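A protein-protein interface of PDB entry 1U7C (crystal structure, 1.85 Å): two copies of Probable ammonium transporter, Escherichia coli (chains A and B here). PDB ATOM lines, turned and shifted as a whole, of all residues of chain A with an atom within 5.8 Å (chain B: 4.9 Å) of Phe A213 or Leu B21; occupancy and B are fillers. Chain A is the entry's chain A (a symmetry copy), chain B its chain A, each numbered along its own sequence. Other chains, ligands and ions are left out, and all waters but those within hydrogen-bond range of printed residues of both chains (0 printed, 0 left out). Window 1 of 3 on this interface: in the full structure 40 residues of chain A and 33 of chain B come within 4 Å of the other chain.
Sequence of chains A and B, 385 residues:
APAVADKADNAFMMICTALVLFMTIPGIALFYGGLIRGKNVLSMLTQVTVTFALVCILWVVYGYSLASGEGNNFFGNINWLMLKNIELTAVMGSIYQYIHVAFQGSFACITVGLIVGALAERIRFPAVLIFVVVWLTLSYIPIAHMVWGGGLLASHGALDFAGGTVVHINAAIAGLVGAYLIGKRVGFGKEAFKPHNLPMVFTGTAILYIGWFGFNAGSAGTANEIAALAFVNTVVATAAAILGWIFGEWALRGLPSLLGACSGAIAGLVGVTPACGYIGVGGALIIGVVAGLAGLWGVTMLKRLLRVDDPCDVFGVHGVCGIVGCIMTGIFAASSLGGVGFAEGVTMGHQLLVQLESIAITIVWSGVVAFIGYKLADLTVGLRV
Among the printed residues, merely in contact across the chains: Tyr A209 with Leu B21 (3.8 Å), Tyr A209 with Ile B25 (3.9 Å), Tyr A209 with Phe B52 (3.2 Å), Ile A210 with Ala B18 (3.6 Å), Ile A210 with Leu B21 (3.7 Å), Ile A210 with Phe B22 (3.3 Å), Ile A210 with Ile B25 (3.4 Å), Phe A213 with Leu B21 (3.4 Å), Phe A231 with Thr B17 (3.5 Å), Phe A231 with Ala B18 (3.7 Å) and Val A235 with Leu B21 (3.98 Å).
Phe A12 touches none of the printed residues of chain B.
Of chain B, only Leu B21 (3.4 Å) comes within 4 Å of Phe A213.
Of the printed residues of chain B, Phe A231 touches Thr B17 and Ala B18.
Val B20 touches none of the printed residues of chain A.
Printed residues of chain A within 4 Å of Leu B21: Tyr A209 (3.8 Å), Ile A210 (3.7 Å), Phe A213 (3.4 Å) and Val A235 (3.98 Å).
Printed residues of chain A within 4 Å of Phe B22: Ile A210.
The nearest printed residue of chain A that does not touch Leu B21 is Phe A231 (4.1 Å).
Of the 12 printed residues of chain B, 6 touch a printed residue of chain A.
Printed residues of chain B that touch a printed residue of chain A: Thr B17, Ala B18, Leu B21, Phe B22, Ile B25 and Phe B52.
Hydrophobic or aromatic side chains of chain B that line the printed part of chain A: Leu B21, Phe B22, Ile B25 and Phe B52.
Among the printed residues, 11 pairs touch across the chains.
Among the printed residues, no Asp or Glu carboxylate lies within 4 Å of a Lys or Arg side-chain nitrogen of the other chain.
1 position is printed for both chains.
Of the 11 pairs that touch across the chains among the printed residues, none has its exchanged pair printed and touching as well.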
ATOM      1  N   PHE A  12      33.945 -23.311 -23.751  1.00  0.00           N
ATOM      2  CA  PHE A  12      32.600 -22.785 -23.598  1.00  0.00           C
ATOM      3  C   PHE A  12      31.618 -23.496 -24.511  1.00  0.00           C
ATOM      4  O   PHE A  12      30.547 -23.924 -24.083  1.00  0.00           O
ATOM      5  CB  PHE A  12      32.581 -21.295 -23.926  1.00  0.00           C
ATOM      6  CG  PHE A  12      31.239 -20.650 -23.755  1.00  0.00           C
ATOM      7  CD1 PHE A  12      30.600 -20.666 -22.519  1.00  0.00           C
ATOM      8  CD2 PHE A  12      30.625 -20.002 -24.822  1.00  0.00           C
ATOM      9  CE1 PHE A  12      29.368 -20.038 -22.350  1.00  0.00           C
ATOM     10  CE2 PHE A  12      29.394 -19.372 -24.661  1.00  0.00           C
ATOM     11  CZ  PHE A  12      28.768 -19.392 -23.422  1.00  0.00           C
ATOM     12  N   CYS A  16      28.492 -25.816 -23.698  1.00  0.00           N
ATOM     13  CA  CYS A  16      27.182 -25.354 -24.147  1.00  0.00           C
ATOM     14  C   CYS A  16      26.520 -26.461 -24.954  1.00  0.00           C
ATOM     15  O   CYS A  16      25.312 -26.646 -24.878  1.00  0.00           O
ATOM     16  CB  CYS A  16      27.293 -24.092 -24.997  1.00  0.00           C
ATOM     17  SG  CYS A  16      27.536 -22.605 -24.028  1.00  0.00           S
ATOM     18  N   LEU A  19      25.139 -28.925 -22.665  1.00  0.00           N
ATOM     19  CA  LEU A  19      23.933 -28.363 -22.074  1.00  0.00           C
ATOM     20  C   LEU A  19      22.755 -28.475 -23.030  1.00  0.00           C
ATOM     21  O   LEU A  19      21.638 -28.771 -22.613  1.00  0.00           O
ATOM     22  CB  LEU A  19      24.163 -26.902 -21.695  1.00  0.00           C
ATOM     23  CG  LEU A  19      25.009 -26.705 -20.433  1.00  0.00           C
ATOM     24  CD1 LEU A  19      25.398 -25.241 -20.287  1.00  0.00           C
ATOM     25  CD2 LEU A  19      24.219 -27.182 -19.219  1.00  0.00           C
ATOM     26  N   LEU A 208      15.438 -28.111 -19.146  1.00  0.00           N
ATOM     27  CA  LEU A 208      15.372 -27.350 -20.386  1.00  0.00           C
ATOM     28  C   LEU A 208      15.912 -25.949 -20.123  1.00  0.00           C
ATOM     29  O   LEU A 208      16.667 -25.413 -20.919  1.00  0.00           O
ATOM     30  CB  LEU A 208      13.929 -27.252 -20.879  1.00  0.00           C
ATOM     31  CG  LEU A 208      13.358 -28.522 -21.508  1.00  0.00           C
ATOM     32  CD1 LEU A 208      11.850 -28.425 -21.596  1.00  0.00           C
ATOM     33  CD2 LEU A 208      13.976 -28.718 -22.889  1.00  0.00           C
ATOM     34  N   TYR A 209      15.513 -25.365 -18.999  1.00  0.00           N
ATOM     35  CA  TYR A 209      15.955 -24.028 -18.625  1.00  0.00           C
ATOM     36  C   TYR A 209      17.475 -23.959 -18.485  1.00  0.00           C
ATOM     37  O   TYR A 209      18.120 -23.089 -19.065  1.00  0.00           O
ATOM     38  CB  TYR A 209      15.292 -23.629 -17.306  1.00  0.00           C
ATOM     39  CG  TYR A 209      15.816 -22.353 -16.697  1.00  0.00           C
ATOM     40  CD1 TYR A 209      15.559 -21.114 -17.281  1.00  0.00           C
ATOM     41  CD2 TYR A 209      16.559 -22.387 -15.517  1.00  0.00           C
ATOM     42  CE1 TYR A 209      16.024 -19.940 -16.695  1.00  0.00           C
ATOM     43  CE2 TYR A 209      17.028 -21.226 -14.928  1.00  0.00           C
ATOM     44  CZ  TYR A 209      16.756 -20.007 -15.519  1.00  0.00           C
ATOM     45  OH  TYR A 209      17.202 -18.853 -14.922  1.00  0.00           O
ATOM     46  N   ILE A 210      18.048 -24.871 -17.709  1.00  0.00           N
ATOM     47  CA  ILE A 210      19.492 -24.856 -17.514  1.00  0.00           C
ATOM     48  C   ILE A 210      20.216 -25.119 -18.831  1.00  0.00           C
ATOM     49  O   ILE A 210      21.183 -24.438 -19.168  1.00  0.00           O
ATOM     50  CB  ILE A 210      19.906 -25.896 -16.454  1.00  0.00           C
ATOM     51  CG1 ILE A 210      19.264 -25.535 -15.111  1.00  0.00           C
ATOM     52  CG2 ILE A 210      21.422 -25.940 -16.311  1.00  0.00           C
ATOM     53  CD1 ILE A 210      19.621 -24.137 -14.593  1.00  0.00           C
ATOM     54  N   GLY A 211      19.728 -26.091 -19.595  1.00  0.00           N
ATOM     55  CA  GLY A 211      20.372 -26.383 -20.858  1.00  0.00           C
ATOM     56  C   GLY A 211      20.225 -25.230 -21.826  1.00  0.00           C
ATOM     57  O   GLY A 211      21.074 -25.021 -22.692  1.00  0.00           O
ATOM     58  N   TRP A 212      19.152 -24.464 -21.664  1.00  0.00           N
ATOM     59  CA  TRP A 212      18.885 -23.339 -22.548  1.00  0.00           C
ATOM     60  C   TRP A 212      19.965 -22.273 -22.485  1.00  0.00           C
ATOM     61  O   TRP A 212      20.088 -21.446 -23.391  1.00  0.00           O
ATOM     62  CB  TRP A 212      17.539 -22.714 -22.210  1.00  0.00           C
ATOM     63  CG  TRP A 212      16.758 -22.300 -23.416  1.00  0.00           C
ATOM     64  CD1 TRP A 212      17.120 -21.375 -24.355  1.00  0.00           C
ATOM     65  CD2 TRP A 212      15.462 -22.771 -23.791  1.00  0.00           C
ATOM     66  NE1 TRP A 212      16.118 -21.237 -25.290  1.00  0.00           N
ATOM     67  CE2 TRP A 212      15.091 -22.080 -24.965  1.00  0.00           C
ATOM     68  CE3 TRP A 212      14.576 -23.708 -23.244  1.00  0.00           C
ATOM     69  CZ2 TRP A 212      13.864 -22.296 -25.603  1.00  0.00           C
ATOM     70  CZ3 TRP A 212      13.352 -23.924 -23.884  1.00  0.00           C
ATOM     71  CH2 TRP A 212      13.014 -23.217 -25.048  1.00  0.00           C
ATOM     72  N   PHE A 213      20.745 -22.261 -21.414  1.00  0.00           N
ATOM     73  CA  PHE A 213      21.813 -21.284 -21.343  1.00  0.00           C
ATOM     74  C   PHE A 213      22.868 -21.663 -22.365  1.00  0.00           C
ATOM     75  O   PHE A 213      23.482 -20.800 -22.981  1.00  0.00           O
ATOM     76  CB  PHE A 213      22.375 -21.215 -19.933  1.00  0.00           C
ATOM     77  CG  PHE A 213      21.464 -20.511 -18.986  1.00  0.00           C
ATOM     78  CD1 PHE A 213      21.310 -19.127 -19.055  1.00  0.00           C
ATOM     79  CD2 PHE A 213      20.689 -21.228 -18.084  1.00  0.00           C
ATOM     80  CE1 PHE A 213      20.393 -18.472 -18.248  1.00  0.00           C
ATOM     81  CE2 PHE A 213      19.763 -20.579 -17.269  1.00  0.00           C
ATOM     82  CZ  PHE A 213      19.614 -19.197 -17.352  1.00  0.00           C
ATOM     83  N   GLY A 214      23.065 -22.964 -22.570  1.00  0.00           N
ATOM     84  CA  GLY A 214      24.035 -23.384 -23.565  1.00  0.00           C
ATOM     85  C   GLY A 214      23.478 -23.061 -24.937  1.00  0.00           C
ATOM     86  O   GLY A 214      24.199 -22.659 -25.851  1.00  0.00           O
ATOM     87  N   PHE A 215      22.165 -23.224 -25.052  1.00  0.00           N
ATOM     88  CA  PHE A 215      21.414 -22.985 -26.277  1.00  0.00           C
ATOM     89  C   PHE A 215      21.509 -21.514 -26.685  1.00  0.00           C
ATOM     90  O   PHE A 215      21.956 -21.189 -27.787  1.00  0.00           O
ATOM     91  CB  PHE A 215      19.963 -23.388 -26.006  1.00  0.00           C
ATOM     92  CG  PHE A 215      19.073 -23.406 -27.212  1.00  0.00           C
ATOM     93  CD1 PHE A 215      18.827 -24.593 -27.894  1.00  0.00           C
ATOM     94  CD2 PHE A 215      18.401 -22.254 -27.608  1.00  0.00           C
ATOM     95  CE1 PHE A 215      17.915 -24.635 -28.948  1.00  0.00           C
ATOM     96  CE2 PHE A 215      17.488 -22.283 -28.659  1.00  0.00           C
ATOM     97  CZ  PHE A 215      17.241 -23.479 -29.328  1.00  0.00           C
ATOM     98  N   ASN A 216      21.098 -20.626 -25.788  1.00  0.00           N
ATOM     99  CA  ASN A 216      21.128 -19.198 -26.076  1.00  0.00           C
ATOM    100  C   ASN A 216      22.506 -18.558 -26.037  1.00  0.00           C
ATOM    101  O   ASN A 216      22.922 -17.929 -27.006  1.00  0.00           O
ATOM    102  CB  ASN A 216      20.192 -18.447 -25.130  1.00  0.00           C
ATOM    103  CG  ASN A 216      18.744 -18.583 -25.528  1.00  0.00           C
ATOM    104  OD1 ASN A 216      18.433 -19.135 -26.585  1.00  0.00           O
ATOM    105  ND2 ASN A 216      17.848 -18.065 -24.700  1.00  0.00           N
ATOM    106  N   ALA A 217      23.219 -18.708 -24.925  1.00  0.00           N
ATOM    107  CA  ALA A 217      24.541 -18.102 -24.820  1.00  0.00           C
ATOM    108  C   ALA A 217      25.528 -18.744 -25.782  1.00  0.00           C
ATOM    109  O   ALA A 217      26.375 -18.064 -26.346  1.00  0.00           O
ATOM    110  CB  ALA A 217      25.062 -18.195 -23.391  1.00  0.00           C
ATOM    111  N   GLY A 218      25.409 -20.051 -25.979  1.00  0.00           N
ATOM    112  CA  GLY A 218      26.312 -20.740 -26.883  1.00  0.00           C
ATOM    113  C   GLY A 218      26.130 -20.276 -28.313  1.00  0.00           C
ATOM    114  O   GLY A 218      27.025 -20.415 -29.141  1.00  0.00           O
ATOM    115  N   ALA A 230      23.238 -12.607 -23.813  1.00  0.00           N
ATOM    116  CA  ALA A 230      22.275 -13.662 -24.082  1.00  0.00           C
ATOM    117  C   ALA A 230      21.967 -14.416 -22.796  1.00  0.00           C
ATOM    118  O   ALA A 230      20.819 -14.766 -22.528  1.00  0.00           O
ATOM    119  CB  ALA A 230      22.830 -14.615 -25.134  1.00  0.00           C
ATOM    120  N   PHE A 231      23.000 -14.657 -21.998  1.00  0.00           N
ATOM    121  CA  PHE A 231      22.824 -15.373 -20.745  1.00  0.00           C
ATOM    122  C   PHE A 231      21.907 -14.592 -19.810  1.00  0.00           C
ATOM    123  O   PHE A 231      20.926 -15.127 -19.295  1.00  0.00           O
ATOM    124  CB  PHE A 231      24.185 -15.596 -20.087  1.00  0.00           C
ATOM    125  CG  PHE A 231      24.159 -16.600 -18.975  1.00  0.00           C
ATOM    126  CD1 PHE A 231      23.480 -16.329 -17.791  1.00  0.00           C
ATOM    127  CD2 PHE A 231      24.783 -17.831 -19.124  1.00  0.00           C
ATOM    128  CE1 PHE A 231      23.421 -17.274 -16.774  1.00  0.00           C
ATOM    129  CE2 PHE A 231      24.728 -18.784 -18.113  1.00  0.00           C
ATOM    130  CZ  PHE A 231      24.043 -18.504 -16.935  1.00  0.00           C
ATOM    131  N   VAL A 232      22.227 -13.323 -19.591  1.00  0.00           N
ATOM    132  CA  VAL A 232      21.422 -12.488 -18.715  1.00  0.00           C
ATOM    133  C   VAL A 232      19.994 -12.353 -19.238  1.00  0.00           C
ATOM    134  O   VAL A 232      19.037 -12.443 -18.475  1.00  0.00           O
ATOM    135  CB  VAL A 232      22.049 -11.093 -18.564  1.00  0.00           C
ATOM    136  CG1 VAL A 232      21.102 -10.166 -17.808  1.00  0.00           C
ATOM    137  CG2 VAL A 232      23.369 -11.214 -17.823  1.00  0.00           C
ATOM    138  N   THR A 234      18.398 -14.410 -20.956  1.00  0.00           N
ATOM    139  CA  THR A 234      17.704 -15.679 -20.808  1.00  0.00           C
ATOM    140  C   THR A 234      17.155 -15.749 -19.387  1.00  0.00           C
ATOM    141  O   THR A 234      16.009 -16.129 -19.173  1.00  0.00           O
ATOM    142  CB  THR A 234      18.644 -16.858 -21.083  1.00  0.00           C
ATOM    143  OG1 THR A 234      19.057 -16.803 -22.451  1.00  0.00           O
ATOM    144  CG2 THR A 234      17.941 -18.178 -20.836  1.00  0.00           C
ATOM    145  N   VAL A 235      17.970 -15.358 -18.417  1.00  0.00           N
ATOM    146  CA  VAL A 235      17.528 -15.364 -17.030  1.00  0.00           C
ATOM    147  C   VAL A 235      16.333 -14.433 -16.872  1.00  0.00           C
ATOM    148  O   VAL A 235      15.312 -14.795 -16.286  1.00  0.00           O
ATOM    149  CB  VAL A 235      18.632 -14.865 -16.081  1.00  0.00           C
ATOM    150  CG1 VAL A 235      18.063 -14.679 -14.679  1.00  0.00           C
ATOM    151  CG2 VAL A 235      19.784 -15.856 -16.056  1.00  0.00           C
ATOM    152  N   THR B  17      27.536 -20.048 -13.353  1.00  0.00           N
ATOM    153  CA  THR B  17      26.246 -19.422 -13.081  1.00  0.00           C
ATOM    154  C   THR B  17      25.120 -20.392 -13.416  1.00  0.00           C
ATOM    155  O   THR B  17      24.165 -20.522 -12.657  1.00  0.00           O
ATOM    156  CB  THR B  17      26.058 -18.137 -13.898  1.00  0.00           C
ATOM    157  OG1 THR B  17      27.093 -17.209 -13.557  1.00  0.00           O
ATOM    158  CG2 THR B  17      24.714 -17.504 -13.578  1.00  0.00           C
ATOM    159  N   ALA B  18      25.235 -21.070 -14.554  1.00  0.00           N
ATOM    160  CA  ALA B  18      24.224 -22.042 -14.943  1.00  0.00           C
ATOM    161  C   ALA B  18      24.139 -23.117 -13.868  1.00  0.00           C
ATOM    162  O   ALA B  18      23.055 -23.557 -13.511  1.00  0.00           O
ATOM    163  CB  ALA B  18      24.577 -22.662 -16.278  1.00  0.00           C
ATOM    164  N   LEU B  19      25.294 -23.528 -13.349  1.00  0.00           N
ATOM    165  CA  LEU B  19      25.331 -24.543 -12.308  1.00  0.00           C
ATOM    166  C   LEU B  19      24.648 -24.049 -11.041  1.00  0.00           C
ATOM    167  O   LEU B  19      23.937 -24.803 -10.380  1.00  0.00           O
ATOM    168  CB  LEU B  19      26.775 -24.937 -12.005  1.00  0.00           C
ATOM    169  CG  LEU B  19      27.417 -25.837 -13.065  1.00  0.00           C
ATOM    170  CD1 LEU B  19      28.912 -25.957 -12.814  1.00  0.00           C
ATOM    171  CD2 LEU B  19      26.747 -27.207 -13.032  1.00  0.00           C
ATOM    172  N   VAL B  20      24.857 -22.786 -10.693  1.00  0.00           N
ATOM    173  CA  VAL B  20      24.212 -22.275  -9.491  1.00  0.00           C
ATOM    174  C   VAL B  20      22.703 -22.178  -9.716  1.00  0.00           C
ATOM    175  O   VAL B  20      21.923 -22.461  -8.814  1.00  0.00           O
ATOM    176  CB  VAL B  20      24.780 -20.907  -9.081  1.00  0.00           C
ATOM    177  CG1 VAL B  20      24.024 -20.376  -7.857  1.00  0.00           C
ATOM    178  CG2 VAL B  20      26.264 -21.053  -8.747  1.00  0.00           C
ATOM    179  N   LEU B  21      22.285 -21.785 -10.918  1.00  0.00           N
ATOM    180  CA  LEU B  21      20.853 -21.703 -11.207  1.00  0.00           C
ATOM    181  C   LEU B  21      20.238 -23.099 -11.103  1.00  0.00           C
ATOM    182  O   LEU B  21      19.122 -23.264 -10.626  1.00  0.00           O
ATOM    183  CB  LEU B  21      20.627 -21.114 -12.602  1.00  0.00           C
ATOM    184  CG  LEU B  21      21.003 -19.637 -12.729  1.00  0.00           C
ATOM    185  CD1 LEU B  21      20.881 -19.194 -14.178  1.00  0.00           C
ATOM    186  CD2 LEU B  21      20.090 -18.802 -11.839  1.00  0.00           C
ATOM    187  N   PHE B  22      20.999 -24.095 -11.547  1.00  0.00           N
ATOM    188  CA  PHE B  22      20.613 -25.508 -11.522  1.00  0.00           C
ATOM    189  C   PHE B  22      20.306 -25.926 -10.080  1.00  0.00           C
ATOM    190  O   PHE B  22      19.452 -26.775  -9.831  1.00  0.00           O
ATOM    191  CB  PHE B  22      21.790 -26.299 -12.110  1.00  0.00           C
ATOM    192  CG  PHE B  22      21.538 -27.767 -12.328  1.00  0.00           C
ATOM    193  CD1 PHE B  22      20.325 -28.239 -12.823  1.00  0.00           C
ATOM    194  CD2 PHE B  22      22.582 -28.672 -12.147  1.00  0.00           C
ATOM    195  CE1 PHE B  22      20.161 -29.592 -13.145  1.00  0.00           C
ATOM    196  CE2 PHE B  22      22.431 -30.018 -12.464  1.00  0.00           C
ATOM    197  CZ  PHE B  22      21.220 -30.479 -12.966  1.00  0.00           C
ATOM    198  N   MET B  23      21.010 -25.318  -9.133  1.00  0.00           N
ATOM    199  CA  MET B  23      20.799 -25.614  -7.719  1.00  0.00           C
ATOM    200  C   MET B  23      19.382 -25.272  -7.294  1.00  0.00           C
ATOM    201  O   MET B  23      18.805 -25.956  -6.462  1.00  0.00           O
ATOM    202  CB  MET B  23      21.773 -24.825  -6.853  1.00  0.00           C
ATOM    203  CG  MET B  23      23.212 -25.213  -7.043  1.00  0.00           C
ATOM    204  SD  MET B  23      24.330 -24.120  -5.947  1.00  0.00           S
ATOM    205  CE  MET B  23      23.947 -24.941  -4.252  1.00  0.00           C
ATOM    206  N   THR B  24      18.827 -24.198  -7.842  1.00  0.00           N
ATOM    207  CA  THR B  24      17.470 -23.823  -7.478  1.00  0.00           C
ATOM    208  C   THR B  24      16.475 -24.534  -8.373  1.00  0.00           C
ATOM    209  O   THR B  24      15.524 -25.155  -7.906  1.00  0.00           O
ATOM    210  CB  THR B  24      17.242 -22.315  -7.627  1.00  0.00           C
ATOM    211  OG1 THR B  24      18.180 -21.609  -6.808  1.00  0.00           O
ATOM    212  CG2 THR B  24      15.825 -21.945  -7.200  1.00  0.00           C
ATOM    213  N   ILE B  25      16.725 -24.433  -9.671  1.00  0.00           N
ATOM    214  CA  ILE B  25      15.878 -25.010 -10.699  1.00  0.00           C
ATOM    215  C   ILE B  25      16.664 -26.132 -11.366  1.00  0.00           C
ATOM    216  O   ILE B  25      17.456 -25.892 -12.272  1.00  0.00           O
ATOM    217  CB  ILE B  25      15.529 -23.916 -11.733  1.00  0.00           C
ATOM    218  CG1 ILE B  25      14.894 -22.716 -11.016  1.00  0.00           C
ATOM    219  CG2 ILE B  25      14.612 -24.471 -12.801  1.00  0.00           C
ATOM    220  CD1 ILE B  25      13.608 -23.040 -10.265  1.00  0.00           C
ATOM    221  N   PHE B  52      11.499 -17.667  -7.667  1.00  0.00           N
ATOM    222  CA  PHE B  52      12.776 -17.697  -8.373  1.00  0.00           C
ATOM    223  C   PHE B  52      12.719 -16.616  -9.448  1.00  0.00           C
ATOM    224  O   PHE B  52      13.643 -15.816  -9.596  1.00  0.00           O
ATOM    225  CB  PHE B  52      12.972 -19.069  -9.024  1.00  0.00           C
ATOM    226  CG  PHE B  52      14.083 -19.112 -10.039  1.00  0.00           C
ATOM    227  CD1 PHE B  52      15.412 -19.148  -9.637  1.00  0.00           C
ATOM    228  CD2 PHE B  52      13.794 -19.112 -11.402  1.00  0.00           C
ATOM    229  CE1 PHE B  52      16.446 -19.187 -10.578  1.00  0.00           C
ATOM    230  CE2 PHE B  52      14.816 -19.150 -12.350  1.00  0.00           C
ATOM    231  CZ  PHE B  52      16.144 -19.187 -11.937  1.00  0.00           C
ATOM    232  N   SER B 106      22.268 -15.565  -9.326  1.00  0.00           N
ATOM    233  CA  SER B 106      21.978 -16.967  -9.069  1.00  0.00           C
ATOM    234  C   SER B 106      22.121 -17.287  -7.586  1.00  0.00           C
ATOM    235  O   SER B 106      21.452 -18.176  -7.075  1.00  0.00           O
ATOM    236  CB  SER B 106      22.876 -17.880  -9.917  1.00  0.00           C
ATOM    237  OG  SER B 106      24.233 -17.806  -9.530  1.00  0.00           O
ATOM    238  N   CYS B 109      19.032 -16.305  -5.880  1.00  0.00           N
ATOM    239  CA  CYS B 109      18.014 -17.297  -6.180  1.00  0.00           C
ATOM    240  C   CYS B 109      18.063 -18.528  -5.301  1.00  0.00           C
ATOM    241  O   CYS B 109      17.041 -18.938  -4.755  1.00  0.00           O
ATOM    242  CB  CYS B 109      18.096 -17.722  -7.648  1.00  0.00           C
ATOM    243  SG  CYS B 109      17.581 -16.428  -8.781  1.00  0.00           S
